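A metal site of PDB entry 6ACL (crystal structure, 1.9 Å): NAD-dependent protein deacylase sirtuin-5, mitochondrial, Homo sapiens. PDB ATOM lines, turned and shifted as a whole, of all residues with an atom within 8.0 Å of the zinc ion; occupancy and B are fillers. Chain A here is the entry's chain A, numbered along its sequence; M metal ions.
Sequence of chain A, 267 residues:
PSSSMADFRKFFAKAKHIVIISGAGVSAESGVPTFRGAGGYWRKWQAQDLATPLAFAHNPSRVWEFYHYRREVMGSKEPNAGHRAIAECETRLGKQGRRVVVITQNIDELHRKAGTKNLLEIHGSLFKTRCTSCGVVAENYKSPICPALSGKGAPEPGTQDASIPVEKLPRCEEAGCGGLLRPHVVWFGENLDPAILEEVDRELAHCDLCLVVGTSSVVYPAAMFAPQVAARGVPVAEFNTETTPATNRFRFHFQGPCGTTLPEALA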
ATOM      1  N   ARG A 130       1.242   8.240  28.578  1.00  0.00           N
ATOM      2  CA  ARG A 130       1.311   7.149  27.605  1.00  0.00           C
ATOM      3  C   ARG A 130      -0.009   7.074  26.843  1.00  0.00           C
ATOM      4  O   ARG A 130      -1.090   7.134  27.472  1.00  0.00           O
ATOM      5  CB  ARG A 130       1.604   5.837  28.310  1.00  0.00           C
ATOM      6  CG  ARG A 130       1.697   4.670  27.344  1.00  0.00           C
ATOM      7  CD  ARG A 130       2.407   3.476  27.935  1.00  0.00           C
ATOM      8  NE  ARG A 130       1.524   2.612  28.716  1.00  0.00           N
ATOM      9  CZ  ARG A 130       1.583   2.431  30.041  1.00  0.00           C
ATOM     10  NH1 ARG A 130       2.437   3.083  30.760  1.00  0.00           N
ATOM     11  NH2 ARG A 130       0.816   1.543  30.654  1.00  0.00           N
ATOM     12  N   CYS A 131       0.033   7.005  25.521  1.00  0.00           N
ATOM     13  CA  CYS A 131      -1.204   6.885  24.762  1.00  0.00           C
ATOM     14  C   CYS A 131      -1.794   5.446  24.859  1.00  0.00           C
ATOM     15  O   CYS A 131      -1.069   4.461  24.568  1.00  0.00           O
ATOM     16  CB  CYS A 131      -0.947   7.313  23.322  1.00  0.00           C
ATOM     17  SG  CYS A 131      -2.432   7.141  22.400  1.00  0.00           S
ATOM     18  N   THR A 132      -3.042   5.276  25.278  1.00  0.00           N
ATOM     19  CA  THR A 132      -3.640   3.950  25.363  1.00  0.00           C
ATOM     20  C   THR A 132      -3.994   3.338  23.988  1.00  0.00           C
ATOM     21  O   THR A 132      -4.348   2.170  23.934  1.00  0.00           O
ATOM     22  CB  THR A 132      -4.949   3.942  26.197  1.00  0.00           C
ATOM     23  OG1 THR A 132      -5.939   4.799  25.598  1.00  0.00           O
ATOM     24  CG2 THR A 132      -4.641   4.421  27.642  1.00  0.00           C
ATOM     25  N   SER A 133      -3.956   4.138  22.929  1.00  0.00           N
ATOM     26  CA  SER A 133      -4.106   3.603  21.550  1.00  0.00           C
ATOM     27  C   SER A 133      -2.757   3.265  20.954  1.00  0.00           C
ATOM     28  O   SER A 133      -2.465   2.112  20.715  1.00  0.00           O
ATOM     29  CB  SER A 133      -4.812   4.607  20.647  1.00  0.00           C
ATOM     30  OG  SER A 133      -6.169   4.646  20.996  1.00  0.00           O
ATOM     31  N   CYS A 134      -1.888   4.257  20.742  1.00  0.00           N
ATOM     32  CA  CYS A 134      -0.603   3.958  20.068  1.00  0.00           C
ATOM     33  C   CYS A 134       0.560   3.575  20.956  1.00  0.00           C
ATOM     34  O   CYS A 134       1.584   3.123  20.475  1.00  0.00           O
ATOM     35  CB  CYS A 134      -0.207   5.137  19.183  1.00  0.00           C
ATOM     36  SG  CYS A 134       0.426   6.581  20.052  1.00  0.00           S
ATOM     37  N   GLY A 135       0.430   3.741  22.270  1.00  0.00           N
ATOM     38  CA  GLY A 135       1.500   3.376  23.192  1.00  0.00           C
ATOM     39  C   GLY A 135       2.666   4.335  23.303  1.00  0.00           C
ATOM     40  O   GLY A 135       3.592   4.072  24.077  1.00  0.00           O
ATOM     41  N   VAL A 136       2.667   5.485  22.615  1.00  0.00           N
ATOM     42  CA  VAL A 136       3.796   6.440  22.720  1.00  0.00           C
ATOM     43  C   VAL A 136       3.846   7.104  24.099  1.00  0.00           C
ATOM     44  O   VAL A 136       2.798   7.501  24.644  1.00  0.00           O
ATOM     45  CB  VAL A 136       3.710   7.577  21.696  1.00  0.00           C
ATOM     46  CG1 VAL A 136       2.462   8.416  21.895  1.00  0.00           C
ATOM     47  CG2 VAL A 136       4.918   8.518  21.807  1.00  0.00           C
ATOM     48  N   VAL A 137       5.047   7.224  24.621  1.00  0.00           N
ATOM     49  CA  VAL A 137       5.297   7.801  25.911  1.00  0.00           C
ATOM     50  C   VAL A 137       5.915   9.181  25.663  1.00  0.00           C
ATOM     51  O   VAL A 137       6.871   9.281  24.881  1.00  0.00           O
ATOM     52  CB  VAL A 137       6.268   6.933  26.729  1.00  0.00           C
ATOM     53  CG1 VAL A 137       6.653   7.638  28.017  1.00  0.00           C
ATOM     54  CG2 VAL A 137       5.622   5.611  27.060  1.00  0.00           C
ATOM     55  N   ARG A 171      -5.489  13.964  25.417  1.00  0.00           N
ATOM     56  CA  ARG A 171      -5.518  13.217  24.134  1.00  0.00           C
ATOM     57  C   ARG A 171      -4.163  13.271  23.447  1.00  0.00           C
ATOM     58  O   ARG A 171      -3.460  14.278  23.514  1.00  0.00           O
ATOM     59  CB  ARG A 171      -6.613  13.749  23.189  1.00  0.00           C
ATOM     60  CG  ARG A 171      -8.047  13.837  23.755  1.00  0.00           C
ATOM     61  CD  ARG A 171      -8.666  12.536  24.296  1.00  0.00           C
ATOM     62  NE  ARG A 171      -8.892  11.515  23.268  1.00  0.00           N
ATOM     63  CZ  ARG A 171      -9.727  10.494  23.374  1.00  0.00           C
ATOM     64  NH1 ARG A 171     -10.508  10.360  24.437  1.00  0.00           N
ATOM     65  NH2 ARG A 171      -9.837   9.626  22.367  1.00  0.00           N
ATOM     66  N   CYS A 172      -3.827  12.201  22.737  1.00  0.00           N
ATOM     67  CA  CYS A 172      -2.541  12.046  22.126  1.00  0.00           C
ATOM     68  C   CYS A 172      -2.392  13.090  21.018  1.00  0.00           C
ATOM     69  O   CYS A 172      -3.314  13.302  20.271  1.00  0.00           O
ATOM     70  CB  CYS A 172      -2.467  10.618  21.520  1.00  0.00           C
ATOM     71  SG  CYS A 172      -0.913  10.190  20.799  1.00  0.00           S
ATOM     72  N   GLU A 173      -1.239  13.710  20.904  1.00  0.00           N
ATOM     73  CA  GLU A 173      -1.009  14.681  19.852  1.00  0.00           C
ATOM     74  C   GLU A 173      -0.197  14.117  18.701  1.00  0.00           C
ATOM     75  O   GLU A 173       0.232  14.865  17.863  1.00  0.00           O
ATOM     76  CB  GLU A 173      -0.354  15.932  20.445  1.00  0.00           C
ATOM     77  CG  GLU A 173      -1.332  16.671  21.375  1.00  0.00           C
ATOM     78  CD  GLU A 173      -0.808  18.024  21.847  1.00  0.00           C
ATOM     79  OE1 GLU A 173       0.397  18.290  21.721  1.00  0.00           O
ATOM     80  OE2 GLU A 173      -1.612  18.834  22.344  1.00  0.00           O
ATOM     81  N   GLU A 174      -0.044  12.809  18.607  1.00  0.00           N
ATOM     82  CA  GLU A 174       0.808  12.272  17.572  1.00  0.00           C
ATOM     83  C   GLU A 174      -0.052  12.451  16.317  1.00  0.00           C
ATOM     84  O   GLU A 174      -1.286  12.381  16.379  1.00  0.00           O
ATOM     85  CB  GLU A 174       1.157  10.817  17.820  1.00  0.00           C
ATOM     86  CG  GLU A 174       2.229  10.587  18.882  1.00  0.00           C
ATOM     87  CD  GLU A 174       3.572  11.178  18.499  1.00  0.00           C
ATOM     88  OE1 GLU A 174       4.136  10.842  17.423  1.00  0.00           O
ATOM     89  OE2 GLU A 174       4.042  12.059  19.247  1.00  0.00           O
ATOM     90  N   ALA A 175       0.578  12.762  15.203  1.00  0.00           N
ATOM     91  CA  ALA A 175      -0.196  12.967  13.975  1.00  0.00           C
ATOM     92  C   ALA A 175      -0.991  11.716  13.649  1.00  0.00           C
ATOM     93  O   ALA A 175      -0.425  10.641  13.528  1.00  0.00           O
ATOM     94  CB  ALA A 175       0.740  13.306  12.828  1.00  0.00           C
ATOM     95  N   GLY A 176      -2.309  11.829  13.540  1.00  0.00           N
ATOM     96  CA  GLY A 176      -3.131  10.652  13.154  1.00  0.00           C
ATOM     97  C   GLY A 176      -3.635   9.731  14.272  1.00  0.00           C
ATOM     98  O   GLY A 176      -4.281   8.719  13.978  1.00  0.00           O
ATOM     99  N   CYS A 177      -3.410  10.088  15.550  1.00  0.00           N
ATOM    100  CA  CYS A 177      -3.802   9.208  16.628  1.00  0.00           C
ATOM    101  C   CYS A 177      -5.090   9.731  17.328  1.00  0.00           C
ATOM    102  O   CYS A 177      -6.159   9.151  17.204  1.00  0.00           O
ATOM    103  CB  CYS A 177      -2.621   8.967  17.616  1.00  0.00           C
ATOM    104  SG  CYS A 177      -3.155   7.810  18.856  1.00  0.00           S
ATOM    105  N   GLY A 178      -4.998  10.789  18.088  1.00  0.00           N
ATOM    106  CA  GLY A 178      -6.156  11.212  18.931  1.00  0.00           C
ATOM    107  C   GLY A 178      -6.567  10.337  20.107  1.00  0.00           C
ATOM    108  O   GLY A 178      -7.607  10.602  20.696  1.00  0.00           O
ATOM    109  N   GLY A 179      -5.820   9.283  20.467  1.00  0.00           N
ATOM    110  CA  GLY A 179      -6.243   8.326  21.533  1.00  0.00           C
ATOM    111  C   GLY A 179      -6.283   8.996  22.933  1.00  0.00           C
ATOM    112  O   GLY A 179      -5.689  10.046  23.155  1.00  0.00           O
ATOM    113  N   LEU A 180      -6.904   8.334  23.878  1.00  0.00           N
ATOM    114  CA  LEU A 180      -6.902   8.774  25.289  1.00  0.00           C
ATOM    115  C   LEU A 180      -5.520   8.511  25.936  1.00  0.00           C
ATOM    116  O   LEU A 180      -5.005   7.386  25.913  1.00  0.00           O
ATOM    117  CB  LEU A 180      -7.931   7.985  26.022  1.00  0.00           C
ATOM    118  CG  LEU A 180      -8.122   8.237  27.525  1.00  0.00           C
ATOM    119  CD1 LEU A 180      -8.478   9.657  27.899  1.00  0.00           C
ATOM    120  CD2 LEU A 180      -9.187   7.316  28.024  1.00  0.00           C
ATOM    121  N   LEU A 181      -4.930   9.538  26.480  1.00  0.00           N
ATOM    122  CA  LEU A 181      -3.754   9.386  27.308  1.00  0.00           C
ATOM    123  C   LEU A 181      -4.080   8.898  28.722  1.00  0.00           C
ATOM    124  O   LEU A 181      -5.130   9.204  29.273  1.00  0.00           O
ATOM    125  CB  LEU A 181      -2.923  10.686  27.387  1.00  0.00           C
ATOM    126  CG  LEU A 181      -2.580  11.335  26.041  1.00  0.00           C
ATOM    127  CD1 LEU A 181      -1.913  12.697  26.224  1.00  0.00           C
ATOM    128  CD2 LEU A 181      -1.702  10.373  25.245  1.00  0.00           C
HETATM  129 ZN    ZN M   1      -1.444   7.938  20.400  1.00  0.00          ZN
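The side-chain sulfur (SG) of Cys 131 sits close to the backbone NH (N) of Ser 133, at 3.4 Å. The backbone carbonyl oxygen (O) of Gly 179 lies within hydrogen-bond range of the backbone NH (N) of Cys 172 (2.9 Å). The backbone NH (N) of Glu 174 sits close to the side-chain sulfur (SG) of Cys 172, at 3.5 Å. SG of Cys 177 sits close to N of Gly 179, 3.4 Å away. The backbone NH (N) of Val 136 sits close to the side-chain sulfur (SG) of Cys 134, at 3.6 Å. The backbone NH of Cys 131 lies within hydrogen-bond range of the backbone carbonyl oxygen of Val 136 (2.9 Å).
The nearest printed residue that does not touch the zinc ion is Val 136 (4.2 Å).
The zinc ion is bound by the side-chain sulfur (SG) of Cys 177 (2.3 Å), the side-chain sulfur (SG) of Cys 134 (2.3 Å), the side-chain sulfur (SG) of Cys 172 (2.3 Å) and the side-chain sulfur (SG) of Cys 131 (2.4 Å). The zinc ion has four donor atoms within binding distance.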
